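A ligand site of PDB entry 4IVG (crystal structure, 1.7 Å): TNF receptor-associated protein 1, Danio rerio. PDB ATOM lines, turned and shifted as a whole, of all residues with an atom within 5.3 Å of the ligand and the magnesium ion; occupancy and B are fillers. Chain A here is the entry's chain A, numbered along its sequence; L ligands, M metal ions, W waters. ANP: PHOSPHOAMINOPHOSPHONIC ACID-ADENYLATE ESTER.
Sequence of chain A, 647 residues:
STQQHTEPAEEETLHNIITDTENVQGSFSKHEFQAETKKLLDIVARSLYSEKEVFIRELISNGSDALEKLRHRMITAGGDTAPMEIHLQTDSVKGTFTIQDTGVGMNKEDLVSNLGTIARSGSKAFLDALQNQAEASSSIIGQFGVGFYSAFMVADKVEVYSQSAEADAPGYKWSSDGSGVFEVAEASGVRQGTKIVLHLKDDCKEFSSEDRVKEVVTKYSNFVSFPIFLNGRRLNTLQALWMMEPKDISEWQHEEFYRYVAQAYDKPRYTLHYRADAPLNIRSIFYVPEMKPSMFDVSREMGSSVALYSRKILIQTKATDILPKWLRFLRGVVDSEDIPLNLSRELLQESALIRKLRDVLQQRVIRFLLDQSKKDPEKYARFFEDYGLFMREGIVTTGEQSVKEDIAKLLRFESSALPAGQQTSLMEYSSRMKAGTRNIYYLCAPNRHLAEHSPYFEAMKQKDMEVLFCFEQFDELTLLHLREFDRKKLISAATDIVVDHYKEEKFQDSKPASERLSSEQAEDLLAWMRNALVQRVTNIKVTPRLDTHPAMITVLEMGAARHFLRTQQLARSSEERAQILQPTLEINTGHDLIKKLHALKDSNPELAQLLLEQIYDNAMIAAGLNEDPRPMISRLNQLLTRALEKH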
ATOM      1  N   GLU A  58      22.587   2.255  23.014  1.00  0.00           N
ATOM      2  CA  GLU A  58      21.480   2.868  22.249  1.00  0.00           C
ATOM      3  C   GLU A  58      21.463   2.407  20.782  1.00  0.00           C
ATOM      4  O   GLU A  58      20.399   2.139  20.214  1.00  0.00           O
ATOM      5  CB  GLU A  58      21.540   4.402  22.364  1.00  0.00           C
ATOM      6  CG  GLU A  58      21.169   4.922  23.759  1.00  0.00           C
ATOM      7  CD  GLU A  58      19.875   4.311  24.260  1.00  0.00           C
ATOM      8  OE1 GLU A  58      18.820   4.530  23.626  1.00  0.00           O
ATOM      9  OE2 GLU A  58      19.931   3.575  25.286  1.00  0.00           O
ATOM     10  N   SER A  61      20.247  -1.178  20.667  1.00  0.00           N
ATOM     11  CA  SER A  61      18.804  -1.240  20.897  1.00  0.00           C
ATOM     12  C   SER A  61      18.055  -0.923  19.599  1.00  0.00           C
ATOM     13  O   SER A  61      17.031  -1.544  19.302  1.00  0.00           O
ATOM     14  CB  SER A  61      18.355  -0.294  22.018  1.00  0.00           C
ATOM     15  OG  SER A  61      18.834  -0.741  23.292  1.00  0.00           O
ATOM     16  N   ASN A  62      18.564   0.034  18.844  1.00  0.00           N
ATOM     17  CA  ASN A  62      17.956   0.405  17.556  1.00  0.00           C
ATOM     18  C   ASN A  62      18.059  -0.709  16.545  1.00  0.00           C
ATOM     19  O   ASN A  62      17.128  -0.959  15.796  1.00  0.00           O
ATOM     20  CB  ASN A  62      18.576   1.707  17.003  1.00  0.00           C
ATOM     21  CG  ASN A  62      18.140   2.920  17.782  1.00  0.00           C
ATOM     22  OD1 ASN A  62      17.152   2.858  18.521  1.00  0.00           O
ATOM     23  ND2 ASN A  62      18.862   4.024  17.625  1.00  0.00           N
ATOM     24  N   GLY A  63      19.200  -1.387  16.554  1.00  0.00           N
ATOM     25  CA  GLY A  63      19.403  -2.529  15.657  1.00  0.00           C
ATOM     26  C   GLY A  63      18.409  -3.613  16.002  1.00  0.00           C
ATOM     27  O   GLY A  63      17.775  -4.208  15.137  1.00  0.00           O
ATOM     28  N   ASP A  65      15.478  -3.296  17.550  1.00  0.00           N
ATOM     29  CA  ASP A  65      14.135  -2.833  17.180  1.00  0.00           C
ATOM     30  C   ASP A  65      13.883  -3.001  15.674  1.00  0.00           C
ATOM     31  O   ASP A  65      12.817  -3.466  15.265  1.00  0.00           O
ATOM     32  CB  ASP A  65      13.948  -1.373  17.615  1.00  0.00           C
ATOM     33  CG  ASP A  65      13.866  -1.224  19.140  1.00  0.00           C
ATOM     34  OD1 ASP A  65      13.733  -2.257  19.828  1.00  0.00           O
ATOM     35  OD2 ASP A  65      13.935  -0.070  19.634  1.00  0.00           O
ATOM     36  N   ALA A  66      14.881  -2.644  14.868  1.00  0.00           N
ATOM     37  CA  ALA A  66      14.759  -2.782  13.399  1.00  0.00           C
ATOM     38  C   ALA A  66      14.610  -4.239  12.985  1.00  0.00           C
ATOM     39  O   ALA A  66      13.898  -4.556  12.043  1.00  0.00           O
ATOM     40  CB  ALA A  66      15.962  -2.167  12.718  1.00  0.00           C
ATOM     41  N   LYS A  69      11.075  -5.564  13.945  1.00  0.00           N
ATOM     42  CA  LYS A  69      10.115  -5.144  12.920  1.00  0.00           C
ATOM     43  C   LYS A  69      10.168  -6.016  11.677  1.00  0.00           C
ATOM     44  O   LYS A  69       9.155  -6.269  11.022  1.00  0.00           O
ATOM     45  CB  LYS A  69      10.352  -3.682  12.536  1.00  0.00           C
ATOM     46  CG  LYS A  69      10.068  -2.721  13.670  1.00  0.00           C
ATOM     47  CD  LYS A  69      10.368  -1.288  13.280  1.00  0.00           C
ATOM     48  CE  LYS A  69      10.362  -0.382  14.511  1.00  0.00           C
ATOM     49  NZ  LYS A  69      10.789   1.001  14.161  1.00  0.00           N
ATOM     50  N   ASP A 101      22.961  -3.552  11.106  1.00  0.00           N
ATOM     51  CA  ASP A 101      21.939  -4.584  11.358  1.00  0.00           C
ATOM     52  C   ASP A 101      21.304  -4.969  10.024  1.00  0.00           C
ATOM     53  O   ASP A 101      21.335  -4.210   9.060  1.00  0.00           O
ATOM     54  CB  ASP A 101      20.864  -4.069  12.322  1.00  0.00           C
ATOM     55  CG  ASP A 101      20.047  -2.914  11.725  1.00  0.00           C
ATOM     56  OD1 ASP A 101      19.186  -3.179  10.876  1.00  0.00           O
ATOM     57  OD2 ASP A 101      20.291  -1.744  12.117  1.00  0.00           O
ATOM     58  N   GLY A 105      15.442  -1.348   7.884  1.00  0.00           N
ATOM     59  CA  GLY A 105      16.011  -0.170   7.232  1.00  0.00           C
ATOM     60  C   GLY A 105      15.046   0.990   7.168  1.00  0.00           C
ATOM     61  O   GLY A 105      13.938   0.953   7.739  1.00  0.00           O
ATOM     62  N   MET A 106      15.455   2.035   6.445  1.00  0.00           N
ATOM     63  CA  MET A 106      14.714   3.277   6.360  1.00  0.00           C
ATOM     64  C   MET A 106      14.729   3.792   4.929  1.00  0.00           C
ATOM     65  O   MET A 106      15.774   3.781   4.271  1.00  0.00           O
ATOM     66  CB  MET A 106      15.356   4.326   7.289  1.00  0.00           C
ATOM     67  CG  MET A 106      15.120   4.086   8.776  1.00  0.00           C
ATOM     68  SD  MET A 106      16.027   5.230   9.821  1.00  0.00           S
ATOM     69  CE  MET A 106      17.671   4.497   9.820  1.00  0.00           C
ATOM     70  N   ASN A 114      12.449  10.377  11.000  1.00  0.00           N
ATOM     71  CA  ASN A 114      12.824   9.706  12.250  1.00  0.00           C
ATOM     72  C   ASN A 114      14.209  10.074  12.801  1.00  0.00           C
ATOM     73  O   ASN A 114      14.362  10.280  14.001  1.00  0.00           O
ATOM     74  CB  ASN A 114      12.654   8.190  12.131  1.00  0.00           C
ATOM     75  CG  ASN A 114      11.216   7.774  11.906  1.00  0.00           C
ATOM     76  OD1 ASN A 114      10.273   8.440  12.347  1.00  0.00           O
ATOM     77  ND2 ASN A 114      11.034   6.652  11.208  1.00  0.00           N
ATOM     78  N   LEU A 115      15.224  10.130  11.936  1.00  0.00           N
ATOM     79  CA  LEU A 115      16.569  10.510  12.388  1.00  0.00           C
ATOM     80  C   LEU A 115      16.689  12.027  12.542  1.00  0.00           C
ATOM     81  O   LEU A 115      17.357  12.514  13.453  1.00  0.00           O
ATOM     82  CB  LEU A 115      17.642  10.008  11.421  1.00  0.00           C
ATOM     83  CG  LEU A 115      17.928   8.503  11.374  1.00  0.00           C
ATOM     84  CD1 LEU A 115      19.214   8.267  10.582  1.00  0.00           C
ATOM     85  CD2 LEU A 115      18.033   7.878  12.764  1.00  0.00           C
ATOM     86  N   ARG A 120      11.163  12.133  18.083  1.00  0.00           N
ATOM     87  CA  ARG A 120      10.239  11.405  17.225  1.00  0.00           C
ATOM     88  C   ARG A 120      10.675   9.963  17.102  1.00  0.00           C
ATOM     89  O   ARG A 120      11.832   9.664  16.771  1.00  0.00           O
ATOM     90  CB  ARG A 120      10.134  12.030  15.834  1.00  0.00           C
ATOM     91  CG  ARG A 120       9.167  11.255  14.968  1.00  0.00           C
ATOM     92  CD  ARG A 120       9.141  11.772  13.568  1.00  0.00           C
ATOM     93  NE  ARG A 120       8.687  13.152  13.552  1.00  0.00           N
ATOM     94  CZ  ARG A 120       7.428  13.519  13.411  1.00  0.00           C
ATOM     95  NH1 ARG A 120       6.485  12.591  13.247  1.00  0.00           N
ATOM     96  NH2 ARG A 120       7.097  14.799  13.421  1.00  0.00           N
ATOM     97  N   SER A 121       9.752   9.043  17.376  1.00  0.00           N
ATOM     98  CA  SER A 121      10.067   7.617  17.388  1.00  0.00           C
ATOM     99  C   SER A 121       9.137   6.860  16.454  1.00  0.00           C
ATOM    100  O   SER A 121       7.942   7.135  16.406  1.00  0.00           O
ATOM    101  CB  SER A 121       9.945   7.083  18.816  1.00  0.00           C
ATOM    102  OG  SER A 121       9.961   5.663  18.834  1.00  0.00           O
ATOM    103  N   GLY A 122       9.681   5.896  15.713  1.00  0.00           N
ATOM    104  CA  GLY A 122       8.857   5.055  14.847  1.00  0.00           C
ATOM    105  C   GLY A 122       8.152   3.917  15.567  1.00  0.00           C
ATOM    106  O   GLY A 122       7.438   3.141  14.939  1.00  0.00           O
ATOM    107  N   SER A 123       8.327   3.817  16.889  1.00  0.00           N
ATOM    108  CA  SER A 123       7.787   2.701  17.676  1.00  0.00           C
ATOM    109  C   SER A 123       6.266   2.618  17.704  1.00  0.00           C
ATOM    110  O   SER A 123       5.688   1.559  17.408  1.00  0.00           O
ATOM    111  CB  SER A 123       8.349   2.720  19.099  1.00  0.00           C
ATOM    112  OG  SER A 123       9.751   2.474  19.102  1.00  0.00           O
ATOM    113  N   ILE A 141      12.287  -1.848  22.254  1.00  0.00           N
ATOM    114  CA  ILE A 141      12.947  -1.169  23.367  1.00  0.00           C
ATOM    115  C   ILE A 141      12.705   0.345  23.364  1.00  0.00           C
ATOM    116  O   ILE A 141      12.417   0.947  24.402  1.00  0.00           O
ATOM    117  CB  ILE A 141      14.473  -1.444  23.325  1.00  0.00           C
ATOM    118  CG1 ILE A 141      14.724  -2.950  23.464  1.00  0.00           C
ATOM    119  CG2 ILE A 141      15.203  -0.626  24.390  1.00  0.00           C
ATOM    120  CD1 ILE A 141      16.069  -3.397  22.820  1.00  0.00           C
ATOM    121  N   GLY A 142      12.766   0.954  22.177  1.00  0.00           N
ATOM    122  CA  GLY A 142      12.745   2.402  22.042  1.00  0.00           C
ATOM    123  C   GLY A 142      11.434   3.059  22.363  1.00  0.00           C
ATOM    124  O   GLY A 142      10.370   2.543  22.008  1.00  0.00           O
ATOM    125  N   GLN A 143      11.494   4.188  23.079  1.00  0.00           N
ATOM    126  CA  GLN A 143      10.270   4.929  23.388  1.00  0.00           C
ATOM    127  C   GLN A 143      10.358   6.466  23.381  1.00  0.00           C
ATOM    128  O   GLN A 143       9.344   7.134  23.226  1.00  0.00           O
ATOM    129  CB  GLN A 143       9.692   4.417  24.726  1.00  0.00           C
ATOM    130  CG  GLN A 143      10.579   4.563  25.926  1.00  0.00           C
ATOM    131  CD  GLN A 143       9.996   3.916  27.176  1.00  0.00           C
ATOM    132  OE1 GLN A 143       9.504   2.786  27.146  1.00  0.00           O
ATOM    133  NE2 GLN A 143      10.026   4.645  28.277  1.00  0.00           N
ATOM    134  N   PHE A 144      11.564   7.002  23.527  1.00  0.00           N
ATOM    135  CA  PHE A 144      11.749   8.446  23.672  1.00  0.00           C
ATOM    136  C   PHE A 144      11.993   9.202  22.370  1.00  0.00           C
ATOM    137  O   PHE A 144      11.610  10.353  22.253  1.00  0.00           O
ATOM    138  CB  PHE A 144      12.903   8.753  24.643  1.00  0.00           C
ATOM    139  CG  PHE A 144      12.675   8.257  26.028  1.00  0.00           C
ATOM    140  CD1 PHE A 144      11.606   8.725  26.776  1.00  0.00           C
ATOM    141  CD2 PHE A 144      13.539   7.329  26.614  1.00  0.00           C
ATOM    142  CE1 PHE A 144      11.366   8.273  28.081  1.00  0.00           C
ATOM    143  CE2 PHE A 144      13.303   6.882  27.931  1.00  0.00           C
ATOM    144  CZ  PHE A 144      12.222   7.354  28.650  1.00  0.00           C
ATOM    145  N   GLY A 145      12.659   8.571  21.414  1.00  0.00           N
ATOM    146  CA  GLY A 145      13.033   9.249  20.185  1.00  0.00           C
ATOM    147  C   GLY A 145      14.323  10.084  20.259  1.00  0.00           C
ATOM    148  O   GLY A 145      14.473  11.040  19.495  1.00  0.00           O
ATOM    149  N   VAL A 146      15.235   9.729  21.170  1.00  0.00           N
ATOM    150  CA  VAL A 146      16.498  10.455  21.352  1.00  0.00           C
ATOM    151  C   VAL A 146      17.757   9.596  21.281  1.00  0.00           C
ATOM    152  O   VAL A 146      18.853  10.137  21.143  1.00  0.00           O
ATOM    153  CB  VAL A 146      16.566  11.256  22.675  1.00  0.00           C
ATOM    154  CG1 VAL A 146      15.359  12.199  22.810  1.00  0.00           C
ATOM    155  CG2 VAL A 146      16.671  10.308  23.878  1.00  0.00           C
ATOM    156  N   GLY A 147      17.599   8.275  21.418  1.00  0.00           N
ATOM    157  CA  GLY A 147      18.742   7.397  21.569  1.00  0.00           C
ATOM    158  C   GLY A 147      19.800   7.524  20.468  1.00  0.00           C
ATOM    159  O   GLY A 147      20.990   7.427  20.722  1.00  0.00           O
ATOM    160  N   PHE A 148      19.362   7.729  19.234  1.00  0.00           N
ATOM    161  CA  PHE A 148      20.321   7.830  18.123  1.00  0.00           C
ATOM    162  C   PHE A 148      21.350   8.957  18.318  1.00  0.00           C
ATOM    163  O   PHE A 148      22.521   8.832  17.910  1.00  0.00           O
ATOM    164  CB  PHE A 148      19.555   8.007  16.814  1.00  0.00           C
ATOM    165  CG  PHE A 148      20.419   8.394  15.638  1.00  0.00           C
ATOM    166  CD1 PHE A 148      21.211   7.457  15.017  1.00  0.00           C
ATOM    167  CD2 PHE A 148      20.410   9.693  15.153  1.00  0.00           C
ATOM    168  CE1 PHE A 148      22.002   7.809  13.927  1.00  0.00           C
ATOM    169  CE2 PHE A 148      21.195  10.041  14.074  1.00  0.00           C
ATOM    170  CZ  PHE A 148      21.982   9.098  13.465  1.00  0.00           C
ATOM    171  N   TYR A 149      20.921  10.062  18.932  1.00  0.00           N
ATOM    172  CA  TYR A 149      21.785  11.243  19.068  1.00  0.00           C
ATOM    173  C   TYR A 149      22.920  11.025  20.049  1.00  0.00           C
ATOM    174  O   TYR A 149      23.880  11.799  20.068  1.00  0.00           O
ATOM    175  CB  TYR A 149      20.959  12.476  19.457  1.00  0.00           C
ATOM    176  CG  TYR A 149      19.856  12.700  18.477  1.00  0.00           C
ATOM    177  CD1 TYR A 149      20.107  13.232  17.214  1.00  0.00           C
ATOM    178  CD2 TYR A 149      18.558  12.327  18.785  1.00  0.00           C
ATOM    179  CE1 TYR A 149      19.078  13.397  16.305  1.00  0.00           C
ATOM    180  CE2 TYR A 149      17.539  12.501  17.901  1.00  0.00           C
ATOM    181  CZ  TYR A 149      17.801  13.027  16.667  1.00  0.00           C
ATOM    182  OH  TYR A 149      16.725  13.174  15.828  1.00  0.00           O
ATOM    183  N   THR A 194      20.614  -1.309   7.898  1.00  0.00           N
ATOM    184  CA  THR A 194      21.203  -0.009   8.232  1.00  0.00           C
ATOM    185  C   THR A 194      22.635  -0.163   8.768  1.00  0.00           C
ATOM    186  O   THR A 194      22.878  -0.940   9.691  1.00  0.00           O
ATOM    187  CB  THR A 194      20.329   0.730   9.277  1.00  0.00           C
ATOM    188  OG1 THR A 194      18.972   0.826   8.787  1.00  0.00           O
ATOM    189  CG2 THR A 194      20.843   2.140   9.571  1.00  0.00           C
ATOM    190  N   ILE A 196      25.788   2.160  10.384  1.00  0.00           N
ATOM    191  CA  ILE A 196      26.132   3.456  10.943  1.00  0.00           C
ATOM    192  C   ILE A 196      27.637   3.516  11.203  1.00  0.00           C
ATOM    193  O   ILE A 196      28.170   2.726  11.984  1.00  0.00           O
ATOM    194  CB  ILE A 196      25.368   3.713  12.253  1.00  0.00           C
ATOM    195  CG1 ILE A 196      23.857   3.640  11.975  1.00  0.00           C
ATOM    196  CG2 ILE A 196      25.740   5.081  12.841  1.00  0.00           C
ATOM    197  CD1 ILE A 196      22.991   3.791  13.255  1.00  0.00           C
ATOM    198  N   ARG A 345      17.630   6.697  30.549  1.00  0.00           N
ATOM    199  CA  ARG A 345      17.430   5.254  30.670  1.00  0.00           C
ATOM    200  C   ARG A 345      18.062   4.656  31.927  1.00  0.00           C
ATOM    201  O   ARG A 345      18.340   3.460  31.989  1.00  0.00           O
ATOM    202  CB  ARG A 345      17.793   4.495  29.386  1.00  0.00           C
ATOM    203  CG  ARG A 345      16.766   4.764  28.277  1.00  0.00           C
ATOM    204  CD  ARG A 345      17.067   4.059  26.952  1.00  0.00           C
ATOM    205  NE  ARG A 345      15.864   4.093  26.126  1.00  0.00           N
ATOM    206  CZ  ARG A 345      14.879   3.196  26.219  1.00  0.00           C
ATOM    207  NH1 ARG A 345      14.992   2.188  27.075  1.00  0.00           N
ATOM    208  NH2 ARG A 345      13.804   3.312  25.460  1.00  0.00           N
HETATM  209  PG  ANP L   1      14.657   5.716  22.247  1.00  0.00           P
HETATM  210  O1G ANP L   1      15.230   7.087  22.383  1.00  0.00           O
HETATM  211  O2G ANP L   1      15.777   4.674  21.870  1.00  0.00           O
HETATM  212  O3G ANP L   1      13.950   5.274  23.595  1.00  0.00           O
HETATM  213  PB  ANP L   1      13.806   5.487  19.494  1.00  0.00           P
HETATM  214  O1B ANP L   1      12.503   5.517  18.745  1.00  0.00           O
HETATM  215  O2B ANP L   1      14.443   4.079  19.231  1.00  0.00           O
HETATM  216  N3B ANP L   1      13.371   5.693  21.116  1.00  0.00           N
HETATM  217  PA  ANP L   1      16.104   6.728  18.381  1.00  0.00           P
HETATM  218  O1A ANP L   1      16.935   5.679  19.033  1.00  0.00           O
HETATM  219  O2A ANP L   1      16.591   8.186  18.394  1.00  0.00           O
HETATM  220  O3A ANP L   1      14.643   6.741  19.105  1.00  0.00           O
HETATM  221  O5' ANP L   1      15.675   6.295  16.907  1.00  0.00           O
HETATM  222  C5' ANP L   1      14.771   7.157  16.177  1.00  0.00           C
HETATM  223  C4' ANP L   1      14.084   6.331  15.113  1.00  0.00           C
HETATM  224  O4' ANP L   1      14.985   6.125  13.996  1.00  0.00           O
HETATM  225  C3' ANP L   1      13.620   4.945  15.501  1.00  0.00           C
HETATM  226  O3' ANP L   1      12.339   4.978  16.137  1.00  0.00           O
HETATM  227  C2' ANP L   1      13.518   4.261  14.137  1.00  0.00           C
HETATM  228  O2' ANP L   1      12.282   4.620  13.502  1.00  0.00           O
HETATM  229  C1' ANP L   1      14.708   4.865  13.394  1.00  0.00           C
HETATM  230  N9  ANP L   1      15.899   4.069  13.461  1.00  0.00           N
HETATM  231  C8  ANP L   1      17.028   4.285  14.243  1.00  0.00           C
HETATM  232  N7  ANP L   1      17.962   3.394  14.105  1.00  0.00           N
HETATM  233  C5  ANP L   1      17.439   2.488  13.172  1.00  0.00           C
HETATM  234  C6  ANP L   1      17.951   1.318  12.596  1.00  0.00           C
HETATM  235  N6  ANP L   1      19.141   0.789  12.893  1.00  0.00           N
HETATM  236  N1  ANP L   1      17.169   0.669  11.699  1.00  0.00           N
HETATM  237  C2  ANP L   1      15.969   1.188  11.401  1.00  0.00           C
HETATM  238  N3  ANP L   1      15.387   2.289  11.868  1.00  0.00           N
HETATM  239  C4  ANP L   1      16.195   2.908  12.772  1.00  0.00           C
HETATM  240 MG    MG M   1      16.426   3.902  20.075  1.00  0.00          MG
HETATM  241  O   HOH W   1      16.244   2.525  23.379  1.00  0.00           O
HETATM  242  O   HOH W   2      15.242   1.253  15.404  1.00  0.00           O
HETATM  243  O   HOH W   3      21.438   1.154  14.990  1.00  0.00           O
HETATM  244  O   HOH W   4      13.906   2.006  17.749  1.00  0.00           O
HETATM  245  O   HOH W   5      16.987   6.349  24.498  1.00  0.00           O
HETATM  246  O   HOH W   6      15.881   2.041  20.764  1.00  0.00           O
HETATM  247  O   HOH W   7      12.625   2.816  11.286  1.00  0.00           O
HETATM  248  O   HOH W   8      13.344   0.485  13.470  1.00  0.00           O
HETATM  249  O   HOH W   9      17.624  -1.308   9.828  1.00  0.00           O
HETATM  250  O   HOH W  10      18.290   3.767  20.981  1.00  0.00           O
HETATM  251  O   HOH W  11      20.533   3.698  15.349  1.00  0.00           O
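N3 of the ligand lies close to SD of Met 106 (3.6 Å).
Residues that only touch the ligand: Glu 58 (3.5 Å), Ala 66 (3.2 Å), Lys 69 (3.97 Å), Leu 115 (3.7 Å), Arg 120 (3.9 Å) and Gly 142 (3.5 Å).
Of the 28 residues printed, 1 comes within 4 Å of the magnesium ion.
OG of Ser 121 is in hydrogen-bond range of O1B of the ligand, at 2.5 Å.
The guanidinium group of Arg 345 lies within salt-bridge range of an oxygen (O3G) of the ligand (2.7 Å).
N of Gln 143 lies within hydrogen-bond range of O3G of the ligand (2.7 Å).
N of Gly 147 is in hydrogen-bond range of O1G of the ligand.
An oxygen (O3') of the ligand lies within hydrogen-bond range of the backbone NH of Gly 122, 2.8 Å away.
The side-chain carboxylate of Asp 101 lies within hydrogen-bond range of a nitrogen (N6) of the ligand (2.9 Å).
N of Val 146 lies within hydrogen-bond range of O1G of the ligand (2.9 Å).
N of Phe 148 sits at hydrogen-bond distance from O2A of the ligand (2.9 Å).
N of Phe 144 sits at hydrogen-bond distance from O3G of the ligand, at 2.9 Å.
The backbone NH (N) of Gly 145 lies within hydrogen-bond range of an oxygen (O1G) of the ligand, 3.1 Å away.
ND2 of Asn 114 is in hydrogen-bond range of O2' of the ligand, 3.3 Å away.
The side-chain hydroxyl (OG1) of Thr 194 lies within hydrogen-bond range of a nitrogen (N1) of the ligand (3.4 Å).
The backbone NH (N) of Ser 123 is in hydrogen-bond range of the side-chain hydroxyl (OG) of Ser 121 (3.1 Å).
The guanidinium group of Arg 345 lies within salt-bridge range of the side-chain carboxylate of Glu 58 (3.9 Å).
The backbone carbonyl oxygen (O) of Ile 141 is in hydrogen-bond range of the guanidinium group (NH2) of Arg 345 (2.9 Å).
The backbone NH (N) of Asp 101 sits at hydrogen-bond distance from the backbone carbonyl oxygen (O) of Thr 194.
The backbone carbonyl oxygen (O) of Gly 142 lies within hydrogen-bond range of the side-chain hydroxyl (OG) of Ser 123, at 3.0 Å.
The backbone NH (N) of Gly 142 sits at hydrogen-bond distance from the side-chain carboxylate (OD2) of Asp 65 (3.0 Å).
The backbone carbonyl oxygen (O) of Leu 115 sits at hydrogen-bond distance from the side-chain hydroxyl (OH) of Tyr 149.
The magnesium ion is bound by the side-chain amide oxygen of Asn 62 (2.0 Å), water W6 (2.1 Å), an oxygen (O2G) of the ligand (2.1 Å), water W10 (2.1 Å), an oxygen (O1A) of the ligand (2.1 Å) and an oxygen (O2B) of the ligand (2.2 Å).
The magnesium ion has six donor atoms within binding distance.
Water W10 lies within hydrogen-bond range of the backbone carbonyl oxygen (O) of Glu 58 (2.8 Å) and the side-chain amide nitrogen (ND2) of Asn 62 (3.4 Å).
Water W1 lies within hydrogen-bond range of the guanidinium group (NE) of Arg 345 and the side-chain carboxylate (OE1) of Glu 58.
Water W9 lies within hydrogen-bond range of OD1 of Asp 101 (2.7 Å), OG1 of Thr 194 (2.7 Å), N1 of the ligand (2.8 Å) and N of Gly 105 (2.9 Å).
Water W5 lies within hydrogen-bond range of OE1 of Glu 58, O1G of the ligand and NE of Arg 345.
Water W11 lies within hydrogen-bond range of the side-chain amide nitrogen of Asn 62 and a nitrogen (N7) of the ligand.
Water W8 bridges the side-chain amino group (NZ) of Lys 69 and a nitrogen (N3) of the ligand.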
